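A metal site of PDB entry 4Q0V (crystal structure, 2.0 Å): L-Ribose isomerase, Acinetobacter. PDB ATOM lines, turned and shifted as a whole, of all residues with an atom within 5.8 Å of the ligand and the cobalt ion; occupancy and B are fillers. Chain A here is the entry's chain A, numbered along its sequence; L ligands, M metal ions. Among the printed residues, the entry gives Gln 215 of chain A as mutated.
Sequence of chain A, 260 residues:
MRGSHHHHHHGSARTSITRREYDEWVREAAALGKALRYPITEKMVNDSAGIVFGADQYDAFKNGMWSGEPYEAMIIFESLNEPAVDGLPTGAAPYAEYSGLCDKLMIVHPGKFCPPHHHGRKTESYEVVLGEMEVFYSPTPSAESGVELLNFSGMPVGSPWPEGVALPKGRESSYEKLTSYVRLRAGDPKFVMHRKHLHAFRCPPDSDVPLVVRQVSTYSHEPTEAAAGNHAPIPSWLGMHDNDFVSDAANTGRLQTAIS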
ATOM      1  N   ILE A  51     -22.460   9.877 -13.763  1.00  0.00           N
ATOM      2  CA  ILE A  51     -23.534  10.852 -13.935  1.00  0.00           C
ATOM      3  C   ILE A  51     -23.065  12.304 -13.886  1.00  0.00           C
ATOM      4  O   ILE A  51     -22.269  12.690 -13.027  1.00  0.00           O
ATOM      5  CB  ILE A  51     -24.615  10.647 -12.845  1.00  0.00           C
ATOM      6  CG1 ILE A  51     -25.039   9.177 -12.803  1.00  0.00           C
ATOM      7  CG2 ILE A  51     -25.838  11.530 -13.125  1.00  0.00           C
ATOM      8  CD1 ILE A  51     -25.751   8.790 -11.521  1.00  0.00           C
ATOM      9  N   PHE A  53     -24.980  15.952 -14.004  1.00  0.00           N
ATOM     10  CA  PHE A  53     -26.323  16.521 -13.953  1.00  0.00           C
ATOM     11  C   PHE A  53     -26.567  17.787 -14.784  1.00  0.00           C
ATOM     12  O   PHE A  53     -26.712  18.887 -14.236  1.00  0.00           O
ATOM     13  CB  PHE A  53     -26.714  16.778 -12.494  1.00  0.00           C
ATOM     14  CG  PHE A  53     -26.672  15.542 -11.613  1.00  0.00           C
ATOM     15  CD1 PHE A  53     -25.488  15.143 -11.011  1.00  0.00           C
ATOM     16  CD2 PHE A  53     -27.816  14.773 -11.410  1.00  0.00           C
ATOM     17  CE1 PHE A  53     -25.436  13.996 -10.201  1.00  0.00           C
ATOM     18  CE2 PHE A  53     -27.783  13.633 -10.610  1.00  0.00           C
ATOM     19  CZ  PHE A  53     -26.599  13.242 -10.002  1.00  0.00           C
ATOM     20  N   MET A  74     -21.271  12.686 -10.396  1.00  0.00           N
ATOM     21  CA  MET A  74     -20.930  11.624  -9.457  1.00  0.00           C
ATOM     22  C   MET A  74     -21.005  10.262 -10.132  1.00  0.00           C
ATOM     23  O   MET A  74     -21.500  10.124 -11.238  1.00  0.00           O
ATOM     24  CB  MET A  74     -21.913  11.619  -8.286  1.00  0.00           C
ATOM     25  CG  MET A  74     -23.306  11.110  -8.689  1.00  0.00           C
ATOM     26  SD  MET A  74     -24.540  11.371  -7.400  1.00  0.00           S
ATOM     27  CE  MET A  74     -24.057  10.101  -6.213  1.00  0.00           C
ATOM     28  N   ILE A  76     -22.158   6.171  -9.513  1.00  0.00           N
ATOM     29  CA  ILE A  76     -23.002   5.293  -8.726  1.00  0.00           C
ATOM     30  C   ILE A  76     -22.952   3.903  -9.333  1.00  0.00           C
ATOM     31  O   ILE A  76     -23.193   3.726 -10.529  1.00  0.00           O
ATOM     32  CB  ILE A  76     -24.470   5.752  -8.707  1.00  0.00           C
ATOM     33  CG1 ILE A  76     -24.602   7.091  -7.960  1.00  0.00           C
ATOM     34  CG2 ILE A  76     -25.337   4.680  -8.062  1.00  0.00           C
ATOM     35  CD1 ILE A  76     -26.027   7.632  -7.901  1.00  0.00           C
ATOM     36  N   LYS A 104     -26.226   0.649  -3.368  1.00  0.00           N
ATOM     37  CA  LYS A 104     -25.374   1.318  -4.344  1.00  0.00           C
ATOM     38  C   LYS A 104     -24.160   1.938  -3.680  1.00  0.00           C
ATOM     39  O   LYS A 104     -24.204   2.331  -2.519  1.00  0.00           O
ATOM     40  CB  LYS A 104     -26.156   2.451  -5.029  1.00  0.00           C
ATOM     41  CG  LYS A 104     -27.517   2.038  -5.532  1.00  0.00           C
ATOM     42  CD  LYS A 104     -28.499   3.206  -5.530  1.00  0.00           C
ATOM     43  CE  LYS A 104     -28.464   3.991  -6.830  1.00  0.00           C
ATOM     44  NZ  LYS A 104     -29.667   4.870  -6.936  1.00  0.00           N
ATOM     45  N   MET A 106     -21.613   5.068  -3.933  1.00  0.00           N
ATOM     46  CA  MET A 106     -21.555   6.389  -4.543  1.00  0.00           C
ATOM     47  C   MET A 106     -20.164   6.969  -4.374  1.00  0.00           C
ATOM     48  O   MET A 106     -19.578   6.925  -3.291  1.00  0.00           O
ATOM     49  CB  MET A 106     -22.599   7.317  -3.904  1.00  0.00           C
ATOM     50  CG  MET A 106     -24.008   6.755  -3.912  1.00  0.00           C
ATOM     51  SD  MET A 106     -25.258   7.902  -3.297  1.00  0.00           S
ATOM     52  CE  MET A 106     -24.726   8.090  -1.580  1.00  0.00           C
ATOM     53  N   CYS A 114     -23.821  15.892  -5.320  1.00  0.00           N
ATOM     54  CA  CYS A 114     -24.940  15.079  -5.754  1.00  0.00           C
ATOM     55  C   CYS A 114     -25.896  16.265  -5.489  1.00  0.00           C
ATOM     56  O   CYS A 114     -26.068  16.679  -4.338  1.00  0.00           O
ATOM     57  CB  CYS A 114     -25.248  13.946  -4.786  1.00  0.00           C
ATOM     58  SG  CYS A 114     -26.781  13.101  -5.199  1.00  0.00           S
ATOM     59  N   HIS A 117     -32.325  17.497  -4.432  1.00  0.00           N
ATOM     60  CA  HIS A 117     -33.443  16.745  -4.983  1.00  0.00           C
ATOM     61  C   HIS A 117     -34.165  16.047  -3.854  1.00  0.00           C
ATOM     62  O   HIS A 117     -33.682  16.026  -2.715  1.00  0.00           O
ATOM     63  CB  HIS A 117     -32.948  15.692  -5.981  1.00  0.00           C
ATOM     64  CG  HIS A 117     -32.182  14.568  -5.341  1.00  0.00           C
ATOM     65  ND1 HIS A 117     -30.851  14.672  -4.991  1.00  0.00           N
ATOM     66  CD2 HIS A 117     -32.573  13.332  -4.940  1.00  0.00           C
ATOM     67  CE1 HIS A 117     -30.453  13.558  -4.406  1.00  0.00           C
ATOM     68  NE2 HIS A 117     -31.481  12.728  -4.360  1.00  0.00           N
ATOM     69  N   HIS A 119     -37.205  12.613  -3.067  1.00  0.00           N
ATOM     70  CA  HIS A 119     -37.899  11.447  -3.589  1.00  0.00           C
ATOM     71  C   HIS A 119     -39.258  11.377  -2.913  1.00  0.00           C
ATOM     72  O   HIS A 119     -39.381  11.650  -1.723  1.00  0.00           O
ATOM     73  CB  HIS A 119     -37.114  10.173  -3.253  1.00  0.00           C
ATOM     74  CG  HIS A 119     -35.680  10.210  -3.698  1.00  0.00           C
ATOM     75  ND1 HIS A 119     -35.317  10.114  -5.020  1.00  0.00           N
ATOM     76  CD2 HIS A 119     -34.539  10.346  -2.997  1.00  0.00           C
ATOM     77  CE1 HIS A 119     -34.002  10.184  -5.117  1.00  0.00           C
ATOM     78  NE2 HIS A 119     -33.504  10.325  -3.896  1.00  0.00           N
ATOM     79  N   LYS A 122     -38.894   6.930  -2.185  1.00  0.00           N
ATOM     80  CA  LYS A 122     -37.655   6.375  -1.641  1.00  0.00           C
ATOM     81  C   LYS A 122     -37.017   7.010  -0.406  1.00  0.00           C
ATOM     82  O   LYS A 122     -36.763   8.217  -0.371  1.00  0.00           O
ATOM     83  CB  LYS A 122     -36.602   6.292  -2.744  1.00  0.00           C
ATOM     84  CG  LYS A 122     -35.293   5.637  -2.303  1.00  0.00           C
ATOM     85  CD  LYS A 122     -34.265   5.601  -3.437  1.00  0.00           C
ATOM     86  CE  LYS A 122     -33.738   6.991  -3.762  1.00  0.00           C
ATOM     87  NZ  LYS A 122     -32.646   6.969  -4.780  1.00  0.00           N
ATOM     88  N   GLU A 124     -33.677   6.832   1.995  1.00  0.00           N
ATOM     89  CA  GLU A 124     -32.255   6.505   1.881  1.00  0.00           C
ATOM     90  C   GLU A 124     -31.534   6.455   3.222  1.00  0.00           C
ATOM     91  O   GLU A 124     -32.034   6.962   4.220  1.00  0.00           O
ATOM     92  CB  GLU A 124     -31.529   7.583   1.077  1.00  0.00           C
ATOM     93  CG  GLU A 124     -31.862   7.633  -0.360  1.00  0.00           C
ATOM     94  CD  GLU A 124     -31.362   8.924  -1.007  1.00  0.00           C
ATOM     95  OE1 GLU A 124     -30.368   9.525  -0.567  1.00  0.00           O
ATOM     96  OE2 GLU A 124     -31.983   9.317  -1.990  1.00  0.00           O
ATOM     97  N   TYR A 126     -27.182   6.477   4.658  1.00  0.00           N
ATOM     98  CA  TYR A 126     -25.784   6.615   4.246  1.00  0.00           C
ATOM     99  C   TYR A 126     -24.785   5.997   5.204  1.00  0.00           C
ATOM    100  O   TYR A 126     -24.900   6.111   6.428  1.00  0.00           O
ATOM    101  CB  TYR A 126     -25.411   8.098   4.085  1.00  0.00           C
ATOM    102  CG  TYR A 126     -26.408   8.946   3.319  1.00  0.00           C
ATOM    103  CD1 TYR A 126     -26.816   8.597   2.043  1.00  0.00           C
ATOM    104  CD2 TYR A 126     -26.943  10.094   3.898  1.00  0.00           C
ATOM    105  CE1 TYR A 126     -27.739   9.385   1.341  1.00  0.00           C
ATOM    106  CE2 TYR A 126     -27.868  10.878   3.218  1.00  0.00           C
ATOM    107  CZ  TYR A 126     -28.266  10.520   1.937  1.00  0.00           C
ATOM    108  OH  TYR A 126     -29.204  11.274   1.283  1.00  0.00           O
ATOM    109  N   HIS A 199     -32.503  16.856  -0.216  1.00  0.00           N
ATOM    110  CA  HIS A 199     -31.164  16.551   0.235  1.00  0.00           C
ATOM    111  C   HIS A 199     -30.137  16.677  -0.881  1.00  0.00           C
ATOM    112  O   HIS A 199     -30.462  16.616  -2.063  1.00  0.00           O
ATOM    113  CB  HIS A 199     -31.086  15.139   0.830  1.00  0.00           C
ATOM    114  CG  HIS A 199     -31.499  14.053  -0.113  1.00  0.00           C
ATOM    115  ND1 HIS A 199     -32.811  13.788  -0.429  1.00  0.00           N
ATOM    116  CD2 HIS A 199     -30.750  13.159  -0.808  1.00  0.00           C
ATOM    117  CE1 HIS A 199     -32.865  12.771  -1.273  1.00  0.00           C
ATOM    118  NE2 HIS A 199     -31.630  12.371  -1.521  1.00  0.00           N
ATOM    119  N   PHE A 201     -25.420  16.468  -1.261  1.00  0.00           N
ATOM    120  CA  PHE A 201     -24.182  16.217  -0.558  1.00  0.00           C
ATOM    121  C   PHE A 201     -22.973  16.406  -1.461  1.00  0.00           C
ATOM    122  O   PHE A 201     -23.073  16.381  -2.680  1.00  0.00           O
ATOM    123  CB  PHE A 201     -24.197  14.812   0.082  1.00  0.00           C
ATOM    124  CG  PHE A 201     -24.421  13.673  -0.880  1.00  0.00           C
ATOM    125  CD1 PHE A 201     -23.352  13.029  -1.484  1.00  0.00           C
ATOM    126  CD2 PHE A 201     -25.718  13.222  -1.144  1.00  0.00           C
ATOM    127  CE1 PHE A 201     -23.570  11.935  -2.338  1.00  0.00           C
ATOM    128  CE2 PHE A 201     -25.936  12.136  -1.992  1.00  0.00           C
ATOM    129  CZ  PHE A 201     -24.867  11.494  -2.583  1.00  0.00           C
ATOM    130  N   GLN A 215     -24.980   3.443  -0.118  1.00  0.00           N
ATOM    131  CA  GLN A 215     -26.363   3.839   0.087  1.00  0.00           C
ATOM    132  C   GLN A 215     -27.282   2.614   0.094  1.00  0.00           C
ATOM    133  O   GLN A 215     -27.266   1.813  -0.845  1.00  0.00           O
ATOM    134  CB  GLN A 215     -26.831   4.784  -1.012  1.00  0.00           C
ATOM    135  CG  GLN A 215     -28.235   5.334  -0.796  1.00  0.00           C
ATOM    136  CD  GLN A 215     -28.870   5.838  -2.083  1.00  0.00           C
ATOM    137  OE1 GLN A 215     -28.239   6.556  -2.848  1.00  0.00           O
ATOM    138  NE2 GLN A 215     -30.115   5.460  -2.314  1.00  0.00           N
ATOM    139  N   SER A 217     -31.233   1.789   0.362  1.00  0.00           N
ATOM    140  CA  SER A 217     -32.513   2.468   0.312  1.00  0.00           C
ATOM    141  C   SER A 217     -33.614   1.559  -0.177  1.00  0.00           C
ATOM    142  O   SER A 217     -33.374   0.405  -0.519  1.00  0.00           O
ATOM    143  CB  SER A 217     -32.413   3.646  -0.646  1.00  0.00           C
ATOM    144  OG  SER A 217     -32.333   3.180  -1.980  1.00  0.00           O
ATOM    145  N   SER A 220     -35.311   1.976  -6.178  1.00  0.00           N
ATOM    146  CA  SER A 220     -34.932   3.175  -6.917  1.00  0.00           C
ATOM    147  C   SER A 220     -35.602   3.201  -8.295  1.00  0.00           C
ATOM    148  O   SER A 220     -35.200   2.498  -9.209  1.00  0.00           O
ATOM    149  CB  SER A 220     -33.406   3.223  -7.058  1.00  0.00           C
ATOM    150  OG  SER A 220     -32.991   4.348  -7.798  1.00  0.00           O
ATOM    151  N   GLU A 222     -35.757   4.707 -11.397  1.00  0.00           N
ATOM    152  CA  GLU A 222     -34.969   5.603 -12.239  1.00  0.00           C
ATOM    153  C   GLU A 222     -34.816   5.095 -13.671  1.00  0.00           C
ATOM    154  O   GLU A 222     -33.903   4.325 -13.961  1.00  0.00           O
ATOM    155  CB  GLU A 222     -33.588   5.809 -11.624  1.00  0.00           C
ATOM    156  CG  GLU A 222     -33.590   6.327 -10.194  1.00  0.00           C
ATOM    157  CD  GLU A 222     -32.186   6.522  -9.633  1.00  0.00           C
ATOM    158  OE1 GLU A 222     -31.453   5.514  -9.507  1.00  0.00           O
ATOM    159  OE2 GLU A 222     -31.810   7.681  -9.348  1.00  0.00           O
ATOM    160  N   ASN A 243     -37.367  10.735  -8.912  1.00  0.00           N
ATOM    161  CA  ASN A 243     -36.360  11.738  -8.600  1.00  0.00           C
ATOM    162  C   ASN A 243     -36.854  13.118  -8.988  1.00  0.00           C
ATOM    163  O   ASN A 243     -37.202  13.358 -10.140  1.00  0.00           O
ATOM    164  CB  ASN A 243     -35.042  11.439  -9.312  1.00  0.00           C
ATOM    165  CG  ASN A 243     -34.513  10.049  -9.013  1.00  0.00           C
ATOM    166  OD1 ASN A 243     -34.691   9.524  -7.913  1.00  0.00           O
ATOM    167  ND2 ASN A 243     -33.830   9.447  -9.987  1.00  0.00           N
ATOM    168  N   PHE A 245     -35.397  16.764  -8.918  1.00  0.00           N
ATOM    169  CA  PHE A 245     -34.291  17.675  -8.687  1.00  0.00           C
ATOM    170  C   PHE A 245     -34.783  19.123  -8.691  1.00  0.00           C
ATOM    171  O   PHE A 245     -35.580  19.527  -9.548  1.00  0.00           O
ATOM    172  CB  PHE A 245     -33.226  17.474  -9.764  1.00  0.00           C
ATOM    173  CG  PHE A 245     -32.461  16.185  -9.628  1.00  0.00           C
ATOM    174  CD1 PHE A 245     -31.317  16.120  -8.837  1.00  0.00           C
ATOM    175  CD2 PHE A 245     -32.906  15.027 -10.267  1.00  0.00           C
ATOM    176  CE1 PHE A 245     -30.628  14.918  -8.683  1.00  0.00           C
ATOM    177  CE2 PHE A 245     -32.217  13.817 -10.119  1.00  0.00           C
ATOM    178  CZ  PHE A 245     -31.072  13.765  -9.330  1.00  0.00           C
ATOM    179  N   ARG A 254     -29.665  13.603 -15.652  1.00  0.00           N
ATOM    180  CA  ARG A 254     -29.578  12.511 -14.699  1.00  0.00           C
ATOM    181  C   ARG A 254     -29.710  11.162 -15.407  1.00  0.00           C
ATOM    182  O   ARG A 254     -28.974  10.218 -15.098  1.00  0.00           O
ATOM    183  CB  ARG A 254     -30.696  12.639 -13.656  1.00  0.00           C
ATOM    184  CG  ARG A 254     -30.448  11.901 -12.343  1.00  0.00           C
ATOM    185  CD  ARG A 254     -30.238  10.415 -12.532  1.00  0.00           C
ATOM    186  NE  ARG A 254     -29.891   9.746 -11.282  1.00  0.00           N
ATOM    187  CZ  ARG A 254     -29.462   8.485 -11.210  1.00  0.00           C
ATOM    188  NH1 ARG A 254     -29.173   7.954 -10.029  1.00  0.00           N
ATOM    189  NH2 ARG A 254     -29.290   7.777 -12.315  1.00  0.00           N
HETATM  190  C1  LIG L   1     -28.734  10.144  -3.618  1.00  0.00           C
HETATM  191  O1  LIG L   1     -29.537  10.951  -2.768  1.00  0.00           O
HETATM  192  C2  LIG L   1     -29.620   9.266  -4.496  1.00  0.00           C
HETATM  193  O2  LIG L   1     -30.846   9.318  -4.400  1.00  0.00           O
HETATM  194  C3  LIG L   1     -28.982   8.276  -5.447  1.00  0.00           C
HETATM  195  O3  LIG L   1     -29.366   6.968  -5.084  1.00  0.00           O
HETATM  196  C4  LIG L   1     -29.432   8.564  -6.884  1.00  0.00           C
HETATM  197  O4  LIG L   1     -30.847   8.461  -6.995  1.00  0.00           O
HETATM  198  C5  LIG L   1     -28.980   9.951  -7.306  1.00  0.00           C
HETATM  199  O5  LIG L   1     -29.377  10.193  -8.647  1.00  0.00           O
HETATM  200 CO    CO M   1     -31.611  10.871  -3.080  1.00  0.00          CO
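An oxygen (O3) of the ligand is in hydrogen-bond range of the side-chain amino group (NZ) of Lys 104. NZ of Lys 122 sits at hydrogen-bond distance from O4 of the ligand (3.2 Å). The guanidinium group (NH1) of Arg 254 is in hydrogen-bond range of an oxygen (O5) of the ligand (2.6 Å). O4 of the ligand is in hydrogen-bond range of OE2 of Glu 222 (2.7 Å). An oxygen (O3) of the ligand is in hydrogen-bond range of the side-chain amide oxygen of Gln 215.
The backbone NH (N) of Gln 215 sits at hydrogen-bond distance from the backbone carbonyl oxygen (O) of Lys 104 (2.8 Å). OG of Ser 220 is in hydrogen-bond range of NZ of Lys 104 (3.5 Å). The side-chain amide nitrogen (ND2) of Asn 243 lies within hydrogen-bond range of the side-chain carboxylate (OE2) of Glu 222, 2.8 Å away. The guanidinium group of Arg 254 is in salt-bridge range of the side-chain carboxylate of Glu 222, at 2.7 Å. A ring nitrogen (ND1) of His 119 lies close to the side-chain amide oxygen (OD1) of Asn 243, at 3.0 Å. The side-chain sulfur (SD) of Met 74 sits at hydrogen-bond distance from the side-chain sulfur (SG) of Cys 114 (3.6 Å). The side-chain hydroxyl of Ser 220 is in hydrogen-bond range of the side-chain carboxylate of Glu 222, 2.6 Å away. OE1 of Glu 222 is in salt-bridge range of NZ of Lys 104 (3.2 Å).
Ile 76 touches the ligand. Cys 114 touches the ligand. Phe 201 touches the ligand (CE2 to C1, 3.8 Å). Hydrophobic or aromatic side chains within 4 Å of the ligand: Ile 76, His 117, His 119, His 199 and Phe 201.
The nearest printed residue that does not touch the cobalt ion is Lys 122 (4.4 Å).
The cobalt ion is bound by OE2 of Glu 124 (1.9 Å), O1 of the ligand (2.1 Å), NE2 of His 119 (2.1 Å), NE2 of His 199 (2.2 Å), O2 of the ligand (2.2 Å) and NE2 of His 117 (2.3 Å).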
